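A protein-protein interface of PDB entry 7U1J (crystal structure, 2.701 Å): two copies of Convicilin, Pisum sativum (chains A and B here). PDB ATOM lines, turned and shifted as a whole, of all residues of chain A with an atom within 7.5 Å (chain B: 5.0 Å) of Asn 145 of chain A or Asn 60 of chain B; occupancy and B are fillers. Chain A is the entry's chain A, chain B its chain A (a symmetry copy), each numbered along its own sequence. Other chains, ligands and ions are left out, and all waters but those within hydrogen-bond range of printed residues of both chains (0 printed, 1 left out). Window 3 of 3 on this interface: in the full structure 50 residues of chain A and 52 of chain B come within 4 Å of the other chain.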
ATOM      1  N   ASN A  63      -6.850   3.395 -11.137  1.00  0.00           N
ATOM      2  CA  ASN A  63      -6.778   3.075  -9.692  1.00  0.00           C
ATOM      3  C   ASN A  63      -8.157   2.863  -9.069  1.00  0.00           C
ATOM      4  O   ASN A  63      -8.205   3.043  -7.861  1.00  0.00           O
ATOM      5  CB  ASN A  63      -6.054   4.120  -8.851  1.00  0.00           C
ATOM      6  CG  ASN A  63      -5.571   3.508  -7.556  1.00  0.00           C
ATOM      7  OD1 ASN A  63      -5.208   2.324  -7.508  1.00  0.00           O
ATOM      8  ND2 ASN A  63      -5.637   4.257  -6.480  1.00  0.00           N
ATOM      9  N   ASP A  83      -5.505  -3.687   0.887  1.00  0.00           N
ATOM     10  CA  ASP A  83      -4.637  -2.493   0.714  1.00  0.00           C
ATOM     11  C   ASP A  83      -5.324  -1.539  -0.257  1.00  0.00           C
ATOM     12  O   ASP A  83      -4.747  -1.183  -1.301  1.00  0.00           O
ATOM     13  CB  ASP A  83      -3.226  -2.872   0.286  1.00  0.00           C
ATOM     14  CG  ASP A  83      -2.556  -3.804   1.251  1.00  0.00           C
ATOM     15  OD1 ASP A  83      -2.944  -3.807   2.411  1.00  0.00           O
ATOM     16  OD2 ASP A  83      -1.652  -4.516   0.810  1.00  0.00           O
ATOM     17  N   ALA A  84      -6.501  -1.080   0.135  1.00  0.00           N
ATOM     18  CA  ALA A  84      -7.356  -0.182  -0.668  1.00  0.00           C
ATOM     19  C   ALA A  84      -8.370   0.477   0.244  1.00  0.00           C
ATOM     20  O   ALA A  84      -8.944  -0.234   1.068  1.00  0.00           O
ATOM     21  CB  ALA A  84      -8.054  -0.973  -1.745  1.00  0.00           C
ATOM     22  N   ILE A 142     -10.136   1.456  -3.975  1.00  0.00           N
ATOM     23  CA  ILE A 142      -9.112   2.495  -4.327  1.00  0.00           C
ATOM     24  C   ILE A 142      -7.809   2.013  -3.698  1.00  0.00           C
ATOM     25  O   ILE A 142      -7.571   2.241  -2.504  1.00  0.00           O
ATOM     26  CB  ILE A 142      -9.558   3.896  -3.818  1.00  0.00           C
ATOM     27  CG1 ILE A 142     -11.058   4.129  -4.028  1.00  0.00           C
ATOM     28  CG2 ILE A 142      -8.738   5.004  -4.437  1.00  0.00           C
ATOM     29  CD1 ILE A 142     -11.546   5.422  -3.458  1.00  0.00           C
ATOM     30  N   PRO A 143      -7.044   1.165  -4.423  1.00  0.00           N
ATOM     31  CA  PRO A 143      -5.732   0.676  -3.977  1.00  0.00           C
ATOM     32  C   PRO A 143      -4.720   1.758  -3.601  1.00  0.00           C
ATOM     33  O   PRO A 143      -4.780   2.802  -4.159  1.00  0.00           O
ATOM     34  CB  PRO A 143      -5.162  -0.008  -5.226  1.00  0.00           C
ATOM     35  CG  PRO A 143      -6.391  -0.512  -5.905  1.00  0.00           C
ATOM     36  CD  PRO A 143      -7.419   0.589  -5.722  1.00  0.00           C
ATOM     37  N   VAL A 144      -3.746   1.385  -2.785  1.00  0.00           N
ATOM     38  CA  VAL A 144      -2.813   2.276  -2.040  1.00  0.00           C
ATOM     39  C   VAL A 144      -1.379   2.044  -2.509  1.00  0.00           C
ATOM     40  O   VAL A 144      -0.506   2.843  -2.154  1.00  0.00           O
ATOM     41  CB  VAL A 144      -2.966   1.961  -0.541  1.00  0.00           C
ATOM     42  CG1 VAL A 144      -1.816   2.439   0.290  1.00  0.00           C
ATOM     43  CG2 VAL A 144      -4.251   2.545  -0.024  1.00  0.00           C
ATOM     44  N   ASN A 145      -1.126   0.968  -3.248  1.00  0.00           N
ATOM     45  CA  ASN A 145       0.235   0.413  -3.472  1.00  0.00           C
ATOM     46  C   ASN A 145       0.637   0.474  -4.954  1.00  0.00           C
ATOM     47  O   ASN A 145       1.815   0.738  -5.244  1.00  0.00           O
ATOM     48  CB  ASN A 145       0.298  -1.021  -2.954  1.00  0.00           C
ATOM     49  CG  ASN A 145       0.841  -1.099  -1.552  1.00  0.00           C
ATOM     50  OD1 ASN A 145       1.525  -0.226  -1.100  1.00  0.00           O
ATOM     51  ND2 ASN A 145       0.570  -2.167  -0.857  1.00  0.00           N
ATOM     52  N   GLY A 146      -0.267   0.166  -5.865  1.00  0.00           N
ATOM     53  CA  GLY A 146       0.008   0.139  -7.303  1.00  0.00           C
ATOM     54  C   GLY A 146      -1.306   0.436  -7.974  1.00  0.00           C
ATOM     55  O   GLY A 146      -2.303  -0.017  -7.466  1.00  0.00           O
ATOM     56  N   PRO A 147      -1.385   1.286  -9.019  1.00  0.00           N
ATOM     57  CA  PRO A 147      -2.674   1.660  -9.580  1.00  0.00           C
ATOM     58  C   PRO A 147      -3.478   0.387  -9.878  1.00  0.00           C
ATOM     59  O   PRO A 147      -2.930  -0.470 -10.558  1.00  0.00           O
ATOM     60  CB  PRO A 147      -2.265   2.423 -10.844  1.00  0.00           C
ATOM     61  CG  PRO A 147      -0.901   1.920 -11.150  1.00  0.00           C
ATOM     62  CD  PRO A 147      -0.267   1.872  -9.772  1.00  0.00           C
ATOM     63  N   GLY A 148      -4.685   0.265  -9.300  1.00  0.00           N
ATOM     64  CA  GLY A 148      -5.624  -0.854  -9.518  1.00  0.00           C
ATOM     65  C   GLY A 148      -5.189  -2.188  -8.914  1.00  0.00           C
ATOM     66  O   GLY A 148      -5.943  -3.179  -9.119  1.00  0.00           O
ATOM     67  N   LYS A 149      -4.034  -2.251  -8.236  1.00  0.00           N
ATOM     68  CA  LYS A 149      -3.463  -3.502  -7.680  1.00  0.00           C
ATOM     69  C   LYS A 149      -4.262  -3.922  -6.443  1.00  0.00           C
ATOM     70  O   LYS A 149      -4.147  -3.305  -5.362  1.00  0.00           O
ATOM     71  CB  LYS A 149      -1.981  -3.319  -7.348  1.00  0.00           C
ATOM     72  CG  LYS A 149      -1.158  -4.596  -7.164  1.00  0.00           C
ATOM     73  CD  LYS A 149      -0.890  -5.384  -8.448  1.00  0.00           C
ATOM     74  CE  LYS A 149       0.505  -5.999  -8.556  1.00  0.00           C
ATOM     75  NZ  LYS A 149       0.724  -7.092  -7.571  1.00  0.00           N
ATOM     76  N   GLU A 151      -4.910  -6.164  -3.437  1.00  0.00           N
ATOM     77  CA  GLU A 151      -4.122  -6.962  -2.483  1.00  0.00           C
ATOM     78  C   GLU A 151      -4.946  -7.212  -1.215  1.00  0.00           C
ATOM     79  O   GLU A 151      -5.377  -6.215  -0.580  1.00  0.00           O
ATOM     80  CB  GLU A 151      -2.895  -6.165  -2.066  1.00  0.00           C
ATOM     81  CG  GLU A 151      -1.932  -5.864  -3.185  1.00  0.00           C
ATOM     82  CD  GLU A 151      -0.934  -4.815  -2.747  1.00  0.00           C
ATOM     83  OE1 GLU A 151      -1.073  -4.311  -1.574  1.00  0.00           O
ATOM     84  OE2 GLU A 151      -0.063  -4.457  -3.586  1.00  0.00           O
ATOM     85  N   PHE A 153      -4.995  -9.562   2.517  1.00  0.00           N
ATOM     86  CA  PHE A 153      -4.126 -10.240   3.496  1.00  0.00           C
ATOM     87  C   PHE A 153      -5.044 -10.913   4.497  1.00  0.00           C
ATOM     88  O   PHE A 153      -5.773 -10.209   5.199  1.00  0.00           O
ATOM     89  CB  PHE A 153      -3.180  -9.223   4.145  1.00  0.00           C
ATOM     90  CG  PHE A 153      -1.982  -8.907   3.294  1.00  0.00           C
ATOM     91  CD1 PHE A 153      -0.970  -9.837   3.142  1.00  0.00           C
ATOM     92  CD2 PHE A 153      -1.903  -7.722   2.594  1.00  0.00           C
ATOM     93  CE1 PHE A 153       0.130  -9.572   2.348  1.00  0.00           C
ATOM     94  CE2 PHE A 153      -0.802  -7.452   1.798  1.00  0.00           C
ATOM     95  CZ  PHE A 153       0.203  -8.381   1.663  1.00  0.00           C
ATOM     96  N   LEU B  57       5.299  -2.243 -10.079  1.00  0.00           N
ATOM     97  CA  LEU B  57       5.168  -2.585  -8.627  1.00  0.00           C
ATOM     98  C   LEU B  57       5.306  -1.368  -7.691  1.00  0.00           C
ATOM     99  O   LEU B  57       4.400  -1.173  -6.847  1.00  0.00           O
ATOM    100  CB  LEU B  57       6.188  -3.667  -8.258  1.00  0.00           C
ATOM    101  CG  LEU B  57       5.744  -4.519  -7.065  1.00  0.00           C
ATOM    102  CD1 LEU B  57       4.477  -5.301  -7.396  1.00  0.00           C
ATOM    103  CD2 LEU B  57       6.843  -5.447  -6.568  1.00  0.00           C
ATOM    104  N   PHE B  58       6.403  -0.613  -7.816  1.00  0.00           N
ATOM    105  CA  PHE B  58       6.655   0.694  -7.150  1.00  0.00           C
ATOM    106  C   PHE B  58       6.321   1.853  -8.095  1.00  0.00           C
ATOM    107  O   PHE B  58       6.901   2.940  -7.948  1.00  0.00           O
ATOM    108  CB  PHE B  58       8.104   0.757  -6.674  1.00  0.00           C
ATOM    109  CG  PHE B  58       8.497  -0.501  -5.953  1.00  0.00           C
ATOM    110  CD1 PHE B  58       7.716  -0.988  -4.917  1.00  0.00           C
ATOM    111  CD2 PHE B  58       9.594  -1.241  -6.355  1.00  0.00           C
ATOM    112  CE1 PHE B  58       8.057  -2.165  -4.272  1.00  0.00           C
ATOM    113  CE2 PHE B  58       9.945  -2.404  -5.683  1.00  0.00           C
ATOM    114  CZ  PHE B  58       9.173  -2.869  -4.657  1.00  0.00           C
ATOM    115  N   GLU B  59       5.337   1.659  -8.975  1.00  0.00           N
ATOM    116  CA  GLU B  59       4.874   2.728  -9.872  1.00  0.00           C
ATOM    117  C   GLU B  59       4.392   3.909  -9.013  1.00  0.00           C
ATOM    118  O   GLU B  59       4.460   5.033  -9.465  1.00  0.00           O
ATOM    119  CB  GLU B  59       3.852   2.173 -10.840  1.00  0.00           C
ATOM    120  CG  GLU B  59       3.558   3.158 -11.937  1.00  0.00           C
ATOM    121  CD  GLU B  59       2.429   2.770 -12.865  1.00  0.00           C
ATOM    122  OE1 GLU B  59       2.025   3.647 -13.653  1.00  0.00           O
ATOM    123  OE2 GLU B  59       1.981   1.589 -12.810  1.00  0.00           O
ATOM    124  N   ASN B  60       3.965   3.670  -7.784  1.00  0.00           N
ATOM    125  CA  ASN B  60       3.551   4.740  -6.838  1.00  0.00           C
ATOM    126  C   ASN B  60       4.742   5.468  -6.216  1.00  0.00           C
ATOM    127  O   ASN B  60       4.506   6.556  -5.695  1.00  0.00           O
ATOM    128  CB  ASN B  60       2.808   4.168  -5.637  1.00  0.00           C
ATOM    129  CG  ASN B  60       1.313   4.311  -5.756  1.00  0.00           C
ATOM    130  OD1 ASN B  60       0.783   4.384  -6.851  1.00  0.00           O
ATOM    131  ND2 ASN B  60       0.635   4.288  -4.626  1.00  0.00           N
ATOM    132  N   LEU B  61       5.928   4.852  -6.165  1.00  0.00           N
ATOM    133  CA  LEU B  61       7.154   5.516  -5.668  1.00  0.00           C
ATOM    134  C   LEU B  61       7.936   6.142  -6.828  1.00  0.00           C
ATOM    135  O   LEU B  61       9.116   6.517  -6.610  1.00  0.00           O
ATOM    136  CB  LEU B  61       8.017   4.490  -4.924  1.00  0.00           C
ATOM    137  CG  LEU B  61       7.355   3.821  -3.727  1.00  0.00           C
ATOM    138  CD1 LEU B  61       8.396   3.126  -2.883  1.00  0.00           C
ATOM    139  CD2 LEU B  61       6.586   4.835  -2.895  1.00  0.00           C
ATOM    140  N   GLN B  62       7.336   6.281  -8.009  1.00  0.00           N
ATOM    141  CA  GLN B  62       8.146   6.625  -9.196  1.00  0.00           C
ATOM    142  C   GLN B  62       8.714   8.034  -9.091  1.00  0.00           C
ATOM    143  O   GLN B  62       9.781   8.256  -9.674  1.00  0.00           O
ATOM    144  CB  GLN B  62       7.345   6.592 -10.479  1.00  0.00           C
ATOM    145  CG  GLN B  62       6.167   7.516 -10.426  1.00  0.00           C
ATOM    146  CD  GLN B  62       5.480   7.469 -11.751  1.00  0.00           C
ATOM    147  OE1 GLN B  62       6.111   7.175 -12.767  1.00  0.00           O
ATOM    148  NE2 GLN B  62       4.209   7.816 -11.725  1.00  0.00           N
ATOM    149  N   TYR B  64       9.818   9.473  -6.216  1.00  0.00           N
ATOM    150  CA  TYR B  64      10.793   9.643  -5.086  1.00  0.00           C
ATOM    151  C   TYR B  64      12.151   9.006  -5.425  1.00  0.00           C
ATOM    152  O   TYR B  64      12.206   7.965  -6.108  1.00  0.00           O
ATOM    153  CB  TYR B  64      10.275   9.032  -3.791  1.00  0.00           C
ATOM    154  CG  TYR B  64       8.933   9.579  -3.424  1.00  0.00           C
ATOM    155  CD1 TYR B  64       7.771   9.109  -4.023  1.00  0.00           C
ATOM    156  CD2 TYR B  64       8.829  10.609  -2.504  1.00  0.00           C
ATOM    157  CE1 TYR B  64       6.533   9.617  -3.668  1.00  0.00           C
ATOM    158  CE2 TYR B  64       7.603  11.161  -2.183  1.00  0.00           C
ATOM    159  CZ  TYR B  64       6.455  10.666  -2.765  1.00  0.00           C
ATOM    160  OH  TYR B  64       5.265  11.242  -2.431  1.00  0.00           O
ATOM    161  N   ILE B 291       3.558   3.714   2.758  1.00  0.00           N
ATOM    162  CA  ILE B 291       4.568   2.938   2.020  1.00  0.00           C
ATOM    163  C   ILE B 291       5.881   3.407   2.599  1.00  0.00           C
ATOM    164  O   ILE B 291       6.105   4.606   2.484  1.00  0.00           O
ATOM    165  CB  ILE B 291       4.466   3.258   0.530  1.00  0.00           C
ATOM    166  CG1 ILE B 291       3.098   2.881  -0.024  1.00  0.00           C
ATOM    167  CG2 ILE B 291       5.609   2.599  -0.218  1.00  0.00           C
ATOM    168  CD1 ILE B 291       2.819   3.466  -1.390  1.00  0.00           C
ATOM    169  N   PRO B 341       5.567  -1.889   1.301  1.00  0.00           N
ATOM    170  CA  PRO B 341       4.306  -1.375   0.790  1.00  0.00           C
ATOM    171  C   PRO B 341       3.218  -1.457   1.854  1.00  0.00           C
ATOM    172  O   PRO B 341       3.254  -2.309   2.702  1.00  0.00           O
ATOM    173  CB  PRO B 341       3.945  -2.358  -0.329  1.00  0.00           C
ATOM    174  CG  PRO B 341       5.282  -2.928  -0.726  1.00  0.00           C
ATOM    175  CD  PRO B 341       5.997  -3.111   0.591  1.00  0.00           C
ATOM    176  N   ALA B 342       2.225  -0.604   1.743  1.00  0.00           N
ATOM    177  CA  ALA B 342       1.149  -0.539   2.743  1.00  0.00           C
ATOM    178  C   ALA B 342       0.601  -1.947   2.954  1.00  0.00           C
ATOM    179  O   ALA B 342       0.481  -2.702   1.992  1.00  0.00           O
ATOM    180  CB  ALA B 342       0.105   0.441   2.313  1.00  0.00           C
ATOM    181  N   HIS B 344       1.674  -4.613   4.179  1.00  0.00           N
ATOM    182  CA  HIS B 344       2.594  -5.773   4.067  1.00  0.00           C
ATOM    183  C   HIS B 344       3.216  -6.037   5.433  1.00  0.00           C
ATOM    184  O   HIS B 344       4.002  -5.226   5.904  1.00  0.00           O
ATOM    185  CB  HIS B 344       3.636  -5.576   2.962  1.00  0.00           C
ATOM    186  CG  HIS B 344       3.063  -5.694   1.585  1.00  0.00           C
ATOM    187  ND1 HIS B 344       1.867  -5.086   1.223  1.00  0.00           N
ATOM    188  CD2 HIS B 344       3.506  -6.338   0.490  1.00  0.00           C
ATOM    189  CE1 HIS B 344       1.613  -5.337  -0.045  1.00  0.00           C
ATOM    190  NE2 HIS B 344       2.605  -6.091  -0.519  1.00  0.00           N
ATOM    191  N   ILE B 361       5.647   7.325   2.736  1.00  0.00           N
ATOM    192  CA  ILE B 361       4.871   7.964   1.632  1.00  0.00           C
ATOM    193  C   ILE B 361       3.383   7.692   1.902  1.00  0.00           C
ATOM    194  O   ILE B 361       3.066   6.699   2.511  1.00  0.00           O
ATOM    195  CB  ILE B 361       5.415   7.437   0.292  1.00  0.00           C
ATOM    196  CG1 ILE B 361       6.753   8.086  -0.032  1.00  0.00           C
ATOM    197  CG2 ILE B 361       4.465   7.666  -0.851  1.00  0.00           C
ATOM    198  CD1 ILE B 361       7.841   7.713   0.871  1.00  0.00           C
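No position is printed for both chains. Of the 15 pairs that touch across the chains among the printed residues, none has its exchanged pair printed and touching as well.
Among the printed residues, pairs that only touch across the chains: Glu 151 of chain A with His 344 of chain B (3.3 Å), Asn 145 of chain A with Pro 341 of chain B (3.3 Å), Pro 147 of chain A with Glu 59 of chain B (3.3 Å), Val 144 of chain A with Ala 342 of chain B (3.4 Å), Asn 145 of chain A with His 344 of chain B (3.4 Å), Val 144 of chain A with Ile 291 of chain B (3.5 Å), Asp 83 of chain A with His 344 of chain B (3.5 Å), Asn 145 of chain A with Leu 57 of chain B (3.6 Å), Asn 145 of chain A with Asn 60 of chain B (3.6 Å), Phe 153 of chain A with His 344 of chain B (3.6 Å), Asn 145 of chain A with Ile 291 of chain B (3.6 Å) and Pro 147 of chain A with Asn 60 of chain B (3.99 Å).
ND2 of Asn 145 of chain A lies within hydrogen-bond range of O of Ala 342 of chain B. The backbone carbonyl oxygen (O) of Ala 342 of chain B lies close to the side-chain carboxylate (OD2) of Asp 83 of chain A, 3.0 Å away. O of Val 144 of chain A lies within hydrogen-bond range of ND2 of Asn 60 of chain B (3.1 Å).
O of Ala 342 of chain B lies within hydrogen-bond range of ND1 of His 344 of chain B, at 2.9 Å. O of Asp 83 of chain A lies within hydrogen-bond range of N of Val 144 of chain A, 3.1 Å away. O of Ile 291 of chain B lies within hydrogen-bond range of N of Ile 361 of chain B, at 2.8 Å. A ring nitrogen (ND1) of His 344 of chain B sits close to the backbone carbonyl oxygen of Pro 341 of chain B, 3.4 Å away. The backbone NH (N) of Asp 83 of chain A lies within hydrogen-bond range of the backbone carbonyl oxygen (O) of Glu 151 of chain A (2.9 Å). The side-chain amide nitrogen of Asn 145 of chain A is in hydrogen-bond range of the side-chain carboxylate of Glu 151 of chain A (2.8 Å).
Of the printed residues of chain B, Glu 151 of chain A touches His 344. Of the printed residues of chain B, Phe 153 of chain A touches His 344. Printed residues of chain A within 4 Å of Glu 59 of chain B: Pro 147 (3.3 Å). Printed residues of chain A within 4 Å of Asn 60 of chain B: Val 144, Asn 145 and Pro 147. Printed residues of chain A within 4 Å of Ala 342 of chain B: Asp 83, Val 144 and Asn 145. Of the printed residues of chain A, His 344 of chain B touches Asp 83, Asn 145, Glu 151 and Phe 153. The nearest printed residue of chain A that does not touch Glu 59 of chain B is Asn 145 of chain A (5.2 Å).
Printed residues of chain A that touch a printed residue of chain B: Asp 83, Val 144, Asn 145, Pro 147, Glu 151 and Phe 153. Hydrophobic or aromatic side chains of chain A that line the printed part of chain B: Val 144, Pro 147 and Phe 153. Of the 12 printed residues of chain B, 7 touch a printed residue of chain A. Hydrophobic or aromatic side chains of chain B within 4 Å of the printed part of chain A: Ile 291, Pro 341, Ala 342 and His 344. Among the printed residues, no Asp or Glu carboxylate lies within 4 Å of a Lys or Arg side-chain nitrogen of the other chain.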
